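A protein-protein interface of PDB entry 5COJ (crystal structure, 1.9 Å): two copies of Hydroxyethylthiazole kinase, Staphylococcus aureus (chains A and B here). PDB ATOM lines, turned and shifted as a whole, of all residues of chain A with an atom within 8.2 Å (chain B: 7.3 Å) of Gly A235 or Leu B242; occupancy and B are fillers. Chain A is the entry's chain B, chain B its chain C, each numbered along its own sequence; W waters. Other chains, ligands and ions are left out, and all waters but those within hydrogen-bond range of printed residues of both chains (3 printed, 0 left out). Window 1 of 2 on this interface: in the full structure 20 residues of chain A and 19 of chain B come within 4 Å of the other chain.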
ATOM      1  N   LEU A 181     -15.478  21.374  31.483  1.00  0.00           N
ATOM      2  CA  LEU A 181     -15.289  22.185  30.259  1.00  0.00           C
ATOM      3  C   LEU A 181     -16.576  22.883  29.827  1.00  0.00           C
ATOM      4  O   LEU A 181     -16.507  23.885  29.161  1.00  0.00           O
ATOM      5  CB  LEU A 181     -14.614  21.433  29.112  1.00  0.00           C
ATOM      6  CG  LEU A 181     -13.128  21.230  29.240  1.00  0.00           C
ATOM      7  CD1 LEU A 181     -12.573  20.280  28.150  1.00  0.00           C
ATOM      8  CD2 LEU A 181     -12.323  22.540  29.270  1.00  0.00           C
ATOM      9  N   ARG A 184     -17.074  26.522  30.516  1.00  0.00           N
ATOM     10  CA  ARG A 184     -16.093  27.407  29.887  1.00  0.00           C
ATOM     11  C   ARG A 184     -16.430  27.598  28.439  1.00  0.00           C
ATOM     12  O   ARG A 184     -15.614  28.206  27.653  1.00  0.00           O
ATOM     13  CB  ARG A 184     -14.718  26.814  30.027  1.00  0.00           C
ATOM     14  CG  ARG A 184     -14.319  26.470  31.445  1.00  0.00           C
ATOM     15  CD  ARG A 184     -14.312  27.696  32.338  1.00  0.00           C
ATOM     16  NE  ARG A 184     -13.199  28.586  32.021  1.00  0.00           N
ATOM     17  CZ  ARG A 184     -11.977  28.384  32.478  1.00  0.00           C
ATOM     18  NH1 ARG A 184     -11.760  27.311  33.273  1.00  0.00           N
ATOM     19  NH2 ARG A 184     -10.980  29.211  32.190  1.00  0.00           N
ATOM     20  N   VAL A 185     -17.645  27.173  28.091  1.00  0.00           N
ATOM     21  CA  VAL A 185     -18.142  27.349  26.759  1.00  0.00           C
ATOM     22  C   VAL A 185     -19.458  28.125  26.800  1.00  0.00           C
ATOM     23  O   VAL A 185     -20.422  27.698  27.368  1.00  0.00           O
ATOM     24  CB  VAL A 185     -18.341  25.957  26.102  1.00  0.00           C
ATOM     25  CG1 VAL A 185     -18.923  26.103  24.737  1.00  0.00           C
ATOM     26  CG2 VAL A 185     -17.026  25.198  26.039  1.00  0.00           C
ATOM     27  N   ASN A 230      -8.223  14.554  20.690  1.00  0.00           N
ATOM     28  CA  ASN A 230      -8.089  15.851  20.040  1.00  0.00           C
ATOM     29  C   ASN A 230      -8.733  17.026  20.818  1.00  0.00           C
ATOM     30  O   ASN A 230      -8.796  18.113  20.293  1.00  0.00           O
ATOM     31  CB  ASN A 230      -8.805  15.758  18.662  1.00  0.00           C
ATOM     32  CG  ASN A 230      -8.210  14.649  17.786  1.00  0.00           C
ATOM     33  OD1 ASN A 230      -7.032  14.634  17.523  1.00  0.00           O
ATOM     34  ND2 ASN A 230      -9.048  13.662  17.449  1.00  0.00           N
ATOM     35  N   CYS A 231      -9.279  16.776  21.998  1.00  0.00           N
ATOM     36  CA  CYS A 231      -9.842  17.853  22.826  1.00  0.00           C
ATOM     37  C   CYS A 231      -8.664  18.460  23.610  1.00  0.00           C
ATOM     38  O   CYS A 231      -8.066  17.810  24.469  1.00  0.00           O
ATOM     39  CB  CYS A 231     -10.885  17.344  23.805  1.00  0.00           C
ATOM     40  SG  CYS A 231     -11.612  18.687  24.819  1.00  0.00           S
ATOM     41  N   GLY A 232      -8.290  19.700  23.292  1.00  0.00           N
ATOM     42  CA  GLY A 232      -7.096  20.301  23.913  1.00  0.00           C
ATOM     43  C   GLY A 232      -7.478  21.421  24.877  1.00  0.00           C
ATOM     44  O   GLY A 232      -6.589  22.142  25.321  1.00  0.00           O
ATOM     45  N   GLY A 233      -8.771  21.652  25.114  1.00  0.00           N
ATOM     46  CA  GLY A 233      -9.256  22.752  25.971  1.00  0.00           C
ATOM     47  C   GLY A 233     -10.643  23.198  25.562  1.00  0.00           C
ATOM     48  O   GLY A 233     -11.272  22.526  24.730  1.00  0.00           O
ATOM     49  N   PRO A 234     -11.131  24.333  26.065  1.00  0.00           N
ATOM     50  CA  PRO A 234     -12.484  24.784  25.805  1.00  0.00           C
ATOM     51  C   PRO A 234     -12.743  25.145  24.360  1.00  0.00           C
ATOM     52  O   PRO A 234     -13.944  25.124  23.888  1.00  0.00           O
ATOM     53  CB  PRO A 234     -12.661  26.045  26.732  1.00  0.00           C
ATOM     54  CG  PRO A 234     -11.300  26.483  26.955  1.00  0.00           C
ATOM     55  CD  PRO A 234     -10.415  25.259  26.960  1.00  0.00           C
ATOM     56  N   GLY A 235     -11.704  25.522  23.630  1.00  0.00           N
ATOM     57  CA  GLY A 235     -11.895  25.916  22.201  1.00  0.00           C
ATOM     58  C   GLY A 235     -12.141  24.713  21.307  1.00  0.00           C
ATOM     59  O   GLY A 235     -13.159  24.675  20.580  1.00  0.00           O
ATOM     60  N   THR A 236     -11.287  23.738  21.388  1.00  0.00           N
ATOM     61  CA  THR A 236     -11.516  22.497  20.608  1.00  0.00           C
ATOM     62  C   THR A 236     -12.655  21.635  21.133  1.00  0.00           C
ATOM     63  O   THR A 236     -13.305  20.885  20.330  1.00  0.00           O
ATOM     64  CB  THR A 236     -10.219  21.703  20.461  1.00  0.00           C
ATOM     65  OG1 THR A 236      -9.587  21.518  21.716  1.00  0.00           O
ATOM     66  CG2 THR A 236      -9.287  22.330  19.441  1.00  0.00           C
ATOM     67  N   PHE A 237     -13.021  21.764  22.399  1.00  0.00           N
ATOM     68  CA  PHE A 237     -14.152  21.049  22.967  1.00  0.00           C
ATOM     69  C   PHE A 237     -15.431  21.332  22.243  1.00  0.00           C
ATOM     70  O   PHE A 237     -16.236  20.430  22.011  1.00  0.00           O
ATOM     71  CB  PHE A 237     -14.298  21.370  24.460  1.00  0.00           C
ATOM     72  CG  PHE A 237     -15.510  20.837  25.093  1.00  0.00           C
ATOM     73  CD1 PHE A 237     -15.583  19.562  25.565  1.00  0.00           C
ATOM     74  CD2 PHE A 237     -16.599  21.674  25.342  1.00  0.00           C
ATOM     75  CE1 PHE A 237     -16.755  19.054  26.215  1.00  0.00           C
ATOM     76  CE2 PHE A 237     -17.773  21.198  25.923  1.00  0.00           C
ATOM     77  CZ  PHE A 237     -17.841  19.880  26.376  1.00  0.00           C
ATOM     78  N   SER A 238     -15.644  22.582  21.886  1.00  0.00           N
ATOM     79  CA  SER A 238     -16.966  22.977  21.319  1.00  0.00           C
ATOM     80  C   SER A 238     -17.364  22.236  19.994  1.00  0.00           C
ATOM     81  O   SER A 238     -18.422  21.556  19.894  1.00  0.00           O
ATOM     82  CB  SER A 238     -17.131  24.524  21.379  1.00  0.00           C
ATOM     83  OG  SER A 238     -18.223  24.909  20.516  1.00  0.00           O
ATOM     84  N   PRO A 239     -16.482  22.238  19.006  1.00  0.00           N
ATOM     85  CA  PRO A 239     -16.728  21.403  17.821  1.00  0.00           C
ATOM     86  C   PRO A 239     -16.853  19.897  18.150  1.00  0.00           C
ATOM     87  O   PRO A 239     -17.690  19.200  17.520  1.00  0.00           O
ATOM     88  CB  PRO A 239     -15.527  21.647  16.942  1.00  0.00           C
ATOM     89  CG  PRO A 239     -15.112  23.078  17.347  1.00  0.00           C
ATOM     90  CD  PRO A 239     -15.342  23.146  18.816  1.00  0.00           C
ATOM     91  N   LEU A 240     -16.045  19.423  19.092  1.00  0.00           N
ATOM     92  CA  LEU A 240     -16.084  17.987  19.472  1.00  0.00           C
ATOM     93  C   LEU A 240     -17.410  17.622  20.197  1.00  0.00           C
ATOM     94  O   LEU A 240     -17.934  16.542  19.998  1.00  0.00           O
ATOM     95  CB  LEU A 240     -14.870  17.557  20.268  1.00  0.00           C
ATOM     96  CG  LEU A 240     -13.556  17.625  19.520  1.00  0.00           C
ATOM     97  CD1 LEU A 240     -12.398  17.427  20.459  1.00  0.00           C
ATOM     98  CD2 LEU A 240     -13.451  16.515  18.464  1.00  0.00           C
ATOM     99  N   LEU A 241     -17.991  18.561  20.943  1.00  0.00           N
ATOM    100  CA  LEU A 241     -19.277  18.324  21.555  1.00  0.00           C
ATOM    101  C   LEU A 241     -20.335  18.161  20.461  1.00  0.00           C
ATOM    102  O   LEU A 241     -21.188  17.231  20.545  1.00  0.00           O
ATOM    103  CB  LEU A 241     -19.632  19.515  22.500  1.00  0.00           C
ATOM    104  CG  LEU A 241     -21.063  19.465  23.019  1.00  0.00           C
ATOM    105  CD1 LEU A 241     -21.307  18.260  23.911  1.00  0.00           C
ATOM    106  CD2 LEU A 241     -21.281  20.752  23.825  1.00  0.00           C
ATOM    107  N   ASN B  24     -20.350  36.021  20.698  1.00  0.00           N
ATOM    108  CA  ASN B  24     -19.969  34.690  21.098  1.00  0.00           C
ATOM    109  C   ASN B  24     -18.483  34.515  21.264  1.00  0.00           C
ATOM    110  O   ASN B  24     -18.044  33.964  22.287  1.00  0.00           O
ATOM    111  CB  ASN B  24     -20.596  33.664  20.102  1.00  0.00           C
ATOM    112  CG  ASN B  24     -20.197  32.258  20.382  1.00  0.00           C
ATOM    113  OD1 ASN B  24     -19.113  31.778  19.937  1.00  0.00           O
ATOM    114  ND2 ASN B  24     -20.941  31.617  21.288  1.00  0.00           N
ATOM    115  N   PHE B  25     -17.707  34.959  20.289  1.00  0.00           N
ATOM    116  CA  PHE B  25     -16.240  34.797  20.383  1.00  0.00           C
ATOM    117  C   PHE B  25     -15.682  35.601  21.539  1.00  0.00           C
ATOM    118  O   PHE B  25     -14.745  35.138  22.231  1.00  0.00           O
ATOM    119  CB  PHE B  25     -15.545  35.149  19.023  1.00  0.00           C
ATOM    120  CG  PHE B  25     -14.112  34.751  18.907  1.00  0.00           C
ATOM    121  CD1 PHE B  25     -13.702  33.468  19.139  1.00  0.00           C
ATOM    122  CD2 PHE B  25     -13.178  35.635  18.445  1.00  0.00           C
ATOM    123  CE1 PHE B  25     -12.356  33.048  18.990  1.00  0.00           C
ATOM    124  CE2 PHE B  25     -11.846  35.253  18.269  1.00  0.00           C
ATOM    125  CZ  PHE B  25     -11.436  33.963  18.558  1.00  0.00           C
ATOM    126  N   THR B  26     -16.217  36.777  21.757  1.00  0.00           N
ATOM    127  CA  THR B  26     -15.780  37.586  22.894  1.00  0.00           C
ATOM    128  C   THR B  26     -16.029  36.869  24.217  1.00  0.00           C
ATOM    129  O   THR B  26     -15.124  36.861  25.094  1.00  0.00           O
ATOM    130  CB  THR B  26     -16.467  38.991  22.837  1.00  0.00           C
ATOM    131  OG1 THR B  26     -16.106  39.644  21.588  1.00  0.00           O
ATOM    132  CG2 THR B  26     -15.903  39.809  23.962  1.00  0.00           C
ATOM    133  N   ALA B  27     -17.254  36.342  24.423  1.00  0.00           N
ATOM    134  CA  ALA B  27     -17.611  35.682  25.619  1.00  0.00           C
ATOM    135  C   ALA B  27     -16.743  34.458  25.819  1.00  0.00           C
ATOM    136  O   ALA B  27     -16.189  34.218  26.883  1.00  0.00           O
ATOM    137  CB  ALA B  27     -19.090  35.297  25.623  1.00  0.00           C
ATOM    138  N   ASN B  28     -16.524  33.714  24.744  1.00  0.00           N
ATOM    139  CA  ASN B  28     -15.624  32.521  24.828  1.00  0.00           C
ATOM    140  C   ASN B  28     -14.164  32.830  25.160  1.00  0.00           C
ATOM    141  O   ASN B  28     -13.521  32.084  25.929  1.00  0.00           O
ATOM    142  CB  ASN B  28     -15.696  31.641  23.587  1.00  0.00           C
ATOM    143  CG  ASN B  28     -16.954  30.803  23.546  1.00  0.00           C
ATOM    144  OD1 ASN B  28     -17.395  30.316  24.572  1.00  0.00           O
ATOM    145  ND2 ASN B  28     -17.615  30.751  22.405  1.00  0.00           N
ATOM    146  N   GLY B  29     -13.610  33.874  24.558  1.00  0.00           N
ATOM    147  CA  GLY B  29     -12.275  34.335  24.900  1.00  0.00           C
ATOM    148  C   GLY B  29     -12.110  34.735  26.371  1.00  0.00           C
ATOM    149  O   GLY B  29     -11.127  34.333  27.034  1.00  0.00           O
ATOM    150  N   LEU B  30     -13.075  35.516  26.884  1.00  0.00           N
ATOM    151  CA  LEU B  30     -13.114  35.850  28.268  1.00  0.00           C
ATOM    152  C   LEU B  30     -13.231  34.605  29.161  1.00  0.00           C
ATOM    153  O   LEU B  30     -12.463  34.488  30.189  1.00  0.00           O
ATOM    154  CB  LEU B  30     -14.208  36.893  28.549  1.00  0.00           C
ATOM    155  CG  LEU B  30     -13.793  38.348  28.186  1.00  0.00           C
ATOM    156  CD1 LEU B  30     -15.016  39.283  28.118  1.00  0.00           C
ATOM    157  CD2 LEU B  30     -12.781  38.867  29.162  1.00  0.00           C
ATOM    158  N   LEU B  31     -14.105  33.663  28.828  1.00  0.00           N
ATOM    159  CA  LEU B  31     -14.206  32.443  29.622  1.00  0.00           C
ATOM    160  C   LEU B  31     -12.877  31.636  29.607  1.00  0.00           C
ATOM    161  O   LEU B  31     -12.492  31.067  30.665  1.00  0.00           O
ATOM    162  CB  LEU B  31     -15.338  31.530  29.161  1.00  0.00           C
ATOM    163  CG  LEU B  31     -16.765  31.987  29.540  1.00  0.00           C
ATOM    164  CD1 LEU B  31     -17.707  31.149  28.697  1.00  0.00           C
ATOM    165  CD2 LEU B  31     -17.015  31.840  31.046  1.00  0.00           C
ATOM    166  N   SER B  32     -12.158  31.641  28.481  1.00  0.00           N
ATOM    167  CA  SER B  32     -10.941  30.861  28.394  1.00  0.00           C
ATOM    168  C   SER B  32      -9.808  31.336  29.309  1.00  0.00           C
ATOM    169  O   SER B  32      -9.033  30.506  29.821  1.00  0.00           O
ATOM    170  CB  SER B  32     -10.505  30.696  26.935  1.00  0.00           C
ATOM    171  OG  SER B  32      -9.832  31.931  26.560  1.00  0.00           O
ATOM    172  N   ILE B  33      -9.724  32.658  29.594  1.00  0.00           N
ATOM    173  CA  ILE B  33      -8.757  33.185  30.530  1.00  0.00           C
ATOM    174  C   ILE B  33      -9.260  33.228  31.998  1.00  0.00           C
ATOM    175  O   ILE B  33      -8.501  33.664  32.863  1.00  0.00           O
ATOM    176  CB  ILE B  33      -8.243  34.581  30.131  1.00  0.00           C
ATOM    177  CG1 ILE B  33      -9.366  35.650  30.074  1.00  0.00           C
ATOM    178  CG2 ILE B  33      -7.543  34.544  28.785  1.00  0.00           C
ATOM    179  CD1 ILE B  33      -8.827  37.061  30.008  1.00  0.00           C
ATOM    180  N   LEU B 191     -12.239  40.876  20.160  1.00  0.00           N
ATOM    181  CA  LEU B 191     -12.009  40.054  21.364  1.00  0.00           C
ATOM    182  C   LEU B 191     -10.877  40.721  22.222  1.00  0.00           C
ATOM    183  O   LEU B 191     -10.957  40.664  23.446  1.00  0.00           O
ATOM    184  CB  LEU B 191     -11.635  38.556  21.052  1.00  0.00           C
ATOM    185  CG  LEU B 191     -10.977  37.776  22.172  1.00  0.00           C
ATOM    186  CD1 LEU B 191     -11.893  37.666  23.401  1.00  0.00           C
ATOM    187  CD2 LEU B 191     -10.592  36.335  21.716  1.00  0.00           C
ATOM    188  N   ALA B 221      -0.527  33.933  22.853  1.00  0.00           N
ATOM    189  CA  ALA B 221      -1.444  32.822  22.605  1.00  0.00           C
ATOM    190  C   ALA B 221      -1.666  32.621  21.114  1.00  0.00           C
ATOM    191  O   ALA B 221      -1.701  31.467  20.636  1.00  0.00           O
ATOM    192  CB  ALA B 221      -2.719  32.981  23.354  1.00  0.00           C
ATOM    193  N   ALA B 225      -0.719  29.197  19.144  1.00  0.00           N
ATOM    194  CA  ALA B 225      -1.780  28.488  18.412  1.00  0.00           C
ATOM    195  C   ALA B 225      -1.453  28.297  16.922  1.00  0.00           C
ATOM    196  O   ALA B 225      -1.683  27.223  16.378  1.00  0.00           O
ATOM    197  CB  ALA B 225      -3.087  29.240  18.547  1.00  0.00           C
ATOM    198  N   PHE B 237      -7.629  27.592  13.462  1.00  0.00           N
ATOM    199  CA  PHE B 237      -6.900  28.513  14.364  1.00  0.00           C
ATOM    200  C   PHE B 237      -7.761  28.983  15.531  1.00  0.00           C
ATOM    201  O   PHE B 237      -7.289  29.088  16.661  1.00  0.00           O
ATOM    202  CB  PHE B 237      -6.370  29.711  13.582  1.00  0.00           C
ATOM    203  CG  PHE B 237      -5.797  30.828  14.456  1.00  0.00           C
ATOM    204  CD1 PHE B 237      -4.520  30.778  14.922  1.00  0.00           C
ATOM    205  CD2 PHE B 237      -6.533  31.926  14.727  1.00  0.00           C
ATOM    206  CE1 PHE B 237      -3.984  31.830  15.690  1.00  0.00           C
ATOM    207  CE2 PHE B 237      -5.989  32.995  15.464  1.00  0.00           C
ATOM    208  CZ  PHE B 237      -4.719  32.894  15.960  1.00  0.00           C
ATOM    209  N   SER B 238      -8.990  29.356  15.281  1.00  0.00           N
ATOM    210  CA  SER B 238      -9.807  30.032  16.308  1.00  0.00           C
ATOM    211  C   SER B 238     -10.081  29.143  17.584  1.00  0.00           C
ATOM    212  O   SER B 238      -9.821  29.563  18.712  1.00  0.00           O
ATOM    213  CB  SER B 238     -11.004  30.670  15.636  1.00  0.00           C
ATOM    214  OG  SER B 238     -12.031  30.922  16.589  1.00  0.00           O
ATOM    215  N   PRO B 239     -10.436  27.814  17.415  1.00  0.00           N
ATOM    216  CA  PRO B 239     -10.509  26.955  18.585  1.00  0.00           C
ATOM    217  C   PRO B 239      -9.165  26.771  19.269  1.00  0.00           C
ATOM    218  O   PRO B 239      -9.110  26.665  20.502  1.00  0.00           O
ATOM    219  CB  PRO B 239     -10.975  25.590  18.007  1.00  0.00           C
ATOM    220  CG  PRO B 239     -11.822  26.024  16.840  1.00  0.00           C
ATOM    221  CD  PRO B 239     -11.111  27.211  16.261  1.00  0.00           C
ATOM    222  N   LEU B 240      -8.099  26.682  18.477  1.00  0.00           N
ATOM    223  CA  LEU B 240      -6.719  26.559  19.023  1.00  0.00           C
ATOM    224  C   LEU B 240      -6.261  27.813  19.779  1.00  0.00           C
ATOM    225  O   LEU B 240      -5.612  27.689  20.819  1.00  0.00           O
ATOM    226  CB  LEU B 240      -5.726  26.151  17.956  1.00  0.00           C
ATOM    227  CG  LEU B 240      -5.939  24.764  17.366  1.00  0.00           C
ATOM    228  CD1 LEU B 240      -5.104  24.573  16.124  1.00  0.00           C
ATOM    229  CD2 LEU B 240      -5.646  23.629  18.346  1.00  0.00           C
ATOM    230  N   LEU B 241      -6.746  28.963  19.409  1.00  0.00           N
ATOM    231  CA  LEU B 241      -6.446  30.224  20.179  1.00  0.00           C
ATOM    232  C   LEU B 241      -7.099  30.145  21.548  1.00  0.00           C
ATOM    233  O   LEU B 241      -6.455  30.456  22.561  1.00  0.00           O
ATOM    234  CB  LEU B 241      -6.915  31.460  19.366  1.00  0.00           C
ATOM    235  CG  LEU B 241      -6.890  32.773  20.137  1.00  0.00           C
ATOM    236  CD1 LEU B 241      -5.457  33.135  20.497  1.00  0.00           C
ATOM    237  CD2 LEU B 241      -7.479  33.843  19.266  1.00  0.00           C
ATOM    238  N   LEU B 242      -8.376  29.760  21.618  1.00  0.00           N
ATOM    239  CA  LEU B 242      -9.039  29.601  22.909  1.00  0.00           C
ATOM    240  C   LEU B 242      -8.334  28.579  23.764  1.00  0.00           C
ATOM    241  O   LEU B 242      -8.242  28.768  24.953  1.00  0.00           O
ATOM    242  CB  LEU B 242     -10.502  29.281  22.690  1.00  0.00           C
ATOM    243  CG  LEU B 242     -11.252  30.349  21.891  1.00  0.00           C
ATOM    244  CD1 LEU B 242     -12.653  29.822  21.572  1.00  0.00           C
ATOM    245  CD2 LEU B 242     -11.433  31.654  22.626  1.00  0.00           C
ATOM    246  N   ASP B 243      -7.988  27.390  23.212  1.00  0.00           N
ATOM    247  CA  ASP B 243      -7.253  26.421  24.010  1.00  0.00           C
ATOM    248  C   ASP B 243      -5.944  27.017  24.605  1.00  0.00           C
ATOM    249  O   ASP B 243      -5.512  26.704  25.702  1.00  0.00           O
ATOM    250  CB  ASP B 243      -6.844  25.221  23.160  1.00  0.00           C
ATOM    251  CG  ASP B 243      -8.018  24.267  22.828  1.00  0.00           C
ATOM    252  OD1 ASP B 243      -9.214  24.591  23.220  1.00  0.00           O
ATOM    253  OD2 ASP B 243      -7.734  23.246  22.126  1.00  0.00           O
ATOM    254  N   THR B 244      -5.204  27.730  23.770  1.00  0.00           N
ATOM    255  CA  THR B 244      -3.879  28.261  24.124  1.00  0.00           C
ATOM    256  C   THR B 244      -4.012  29.359  25.214  1.00  0.00           C
ATOM    257  O   THR B 244      -3.188  29.399  26.113  1.00  0.00           O
ATOM    258  CB  THR B 244      -3.162  28.824  22.888  1.00  0.00           C
ATOM    259  OG1 THR B 244      -3.036  27.770  21.893  1.00  0.00           O
ATOM    260  CG2 THR B 244      -1.760  29.250  23.257  1.00  0.00           C
ATOM    261  N   LEU B 245      -5.026  30.187  25.119  1.00  0.00           N
ATOM    262  CA  LEU B 245      -5.336  31.138  26.188  1.00  0.00           C
ATOM    263  C   LEU B 245      -5.628  30.411  27.512  1.00  0.00           C
ATOM    264  O   LEU B 245      -5.202  30.827  28.586  1.00  0.00           O
ATOM    265  CB  LEU B 245      -6.539  31.985  25.819  1.00  0.00           C
ATOM    266  CG  LEU B 245      -6.348  33.026  24.759  1.00  0.00           C
ATOM    267  CD1 LEU B 245      -7.637  33.634  24.216  1.00  0.00           C
ATOM    268  CD2 LEU B 245      -5.472  34.150  25.365  1.00  0.00           C
ATOM    269  N   TYR B 246      -6.401  29.307  27.442  1.00  0.00           N
ATOM    270  CA  TYR B 246      -6.761  28.539  28.620  1.00  0.00           C
ATOM    271  C   TYR B 246      -5.517  27.942  29.280  1.00  0.00           C
ATOM    272  O   TYR B 246      -5.480  27.849  30.519  1.00  0.00           O
ATOM    273  CB  TYR B 246      -7.730  27.404  28.163  1.00  0.00           C
ATOM    274  CG  TYR B 246      -8.162  26.399  29.175  1.00  0.00           C
ATOM    275  CD1 TYR B 246      -9.146  26.685  30.072  1.00  0.00           C
ATOM    276  CD2 TYR B 246      -7.585  25.114  29.229  1.00  0.00           C
ATOM    277  CE1 TYR B 246      -9.594  25.695  30.968  1.00  0.00           C
ATOM    278  CE2 TYR B 246      -8.061  24.114  30.088  1.00  0.00           C
ATOM    279  CZ  TYR B 246      -9.024  24.481  31.008  1.00  0.00           C
ATOM    280  OH  TYR B 246      -9.421  23.500  31.879  1.00  0.00           O
ATOM    281  N   HIS B 247      -4.562  27.421  28.486  1.00  0.00           N
ATOM    282  CA  HIS B 247      -3.369  26.761  29.010  1.00  0.00           C
ATOM    283  C   HIS B 247      -2.139  27.658  29.267  1.00  0.00           C
ATOM    284  O   HIS B 247      -1.147  27.200  29.814  1.00  0.00           O
ATOM    285  CB  HIS B 247      -2.913  25.647  28.073  1.00  0.00           C
ATOM    286  CG  HIS B 247      -3.822  24.467  28.077  1.00  0.00           C
ATOM    287  ND1 HIS B 247      -3.942  23.632  29.166  1.00  0.00           N
ATOM    288  CD2 HIS B 247      -4.689  24.011  27.146  1.00  0.00           C
ATOM    289  CE1 HIS B 247      -4.776  22.637  28.869  1.00  0.00           C
ATOM    290  NE2 HIS B 247      -5.264  22.863  27.660  1.00  0.00           N
ATOM    291  N   LEU B 248      -2.176  28.886  28.794  1.00  0.00           N
ATOM    292  CA  LEU B 248      -0.941  29.733  28.763  1.00  0.00           C
ATOM    293  C   LEU B 248      -0.309  29.764  30.165  1.00  0.00           C
ATOM    294  O   LEU B 248      -0.999  30.090  31.168  1.00  0.00           O
ATOM    295  CB  LEU B 248      -1.267  31.156  28.299  1.00  0.00           C
ATOM    296  CG  LEU B 248      -0.037  32.033  28.045  1.00  0.00           C
ATOM    297  CD1 LEU B 248       0.788  31.472  26.900  1.00  0.00           C
ATOM    298  CD2 LEU B 248      -0.387  33.453  27.777  1.00  0.00           C
HETATM  299  O   HOH W   1     -13.890  29.236  25.894  1.00  0.00           O
HETATM  300  O   HOH W   2      -6.735  20.396  28.030  1.00  0.00           O
HETATM  301  O   HOH W   3     -14.182  31.511  33.199  1.00  0.00           O
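Hydrophobic or aromatic side chains of chain B within 4 Å of the printed part of chain A: Leu B31, Pro B239, Leu B242, Tyr B246 and His B247. Hydrophobic or aromatic side chains of chain A that line the printed part of chain B: Pro A234. Among the printed residues, 15 pairs touch across the chains. Among the printed residues, no Asp or Glu carboxylate lies within 4 Å of a Lys or Arg side-chain nitrogen of the other chain.
Among the printed residues, merely in contact across the chains: Gly A232 with Asp B243 (3.3 Å), Gly A235 with Pro B239 (3.3 Å), Pro A234 with Tyr B246 (3.4 Å), Arg A184 with Tyr B246 (3.6 Å), Gly A235 with Leu B242 (3.7 Å), Val A185 with Asn B28 (3.7 Å), Thr A236 with Pro B239 (3.8 Å) and Val A185 with Leu B31 (3.98 Å).
O of Leu B31 is in hydrogen-bond range of NH2 of Arg A184, at 2.8 Å. The backbone carbonyl oxygen of Ser B32 is in hydrogen-bond range of the guanidinium group of Arg A184, at 3.3 Å. NE2 of His B247 is in hydrogen-bond range of O of Gly A232, at 2.8 Å. The backbone NH (N) of Gly A235 is in hydrogen-bond range of the side-chain carboxylate (OD1) of Asp B243 (2.7 Å). The side-chain hydroxyl of Thr A236 lies within hydrogen-bond range of the side-chain carboxylate of Asp B243, 2.6 Å away. O of Gly A233 lies close to OD1 of Asp B243. OD1 of Asp B243 sits close to N of Pro A234 (3.4 Å).
Water W1 bridges the backbone carbonyl oxygen of Arg A184 (2.7 Å) and the backbone carbonyl oxygen of Asn B28 (2.9 Å). Water W2 bridges a ring nitrogen (NE2) of His B247 (2.9 Å) and the backbone carbonyl oxygen of Gly A232 (3.2 Å). Water W3 bridges the backbone carbonyl oxygen (O) of Leu B31 and the guanidinium group (NE) of Arg A184.
The side-chain hydroxyl of Thr A236 sits at hydrogen-bond distance from the backbone NH of Gly A232 (2.7 Å). The backbone NH (N) of Gly A233 lies within hydrogen-bond range of the side-chain hydroxyl (OG1) of Thr A236. OD1 of Asn B24 is in hydrogen-bond range of ND2 of Asn B28, at 3.1 Å. The backbone carbonyl oxygen (O) of Gly B29 sits at hydrogen-bond distance from the side-chain hydroxyl (OG) of Ser B32, at 2.8 Å.
5 positions are printed for both chains.
Of the printed residues of chain B, Gly A232 touches Asp B243 (3.3 Å) and His B247 (2.8 Å). Of the printed residues of chain B, Pro A234 touches Asp B243 and Tyr B246. Of chain B, only Pro B239, Leu B242 and Asp B243 come within 4 Å of Gly A235. Leu A241 touches none of the printed residues of chain B. Leu B242 touches just one residue of chain A: Gly A235. Of the printed residues of chain A, Asp B243 touches Gly A232, Gly A233, Pro A234, Gly A235 and Thr A236. The nearest residue of chain A that does not touch Leu B242 is Pro A234 (4.3 Å).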
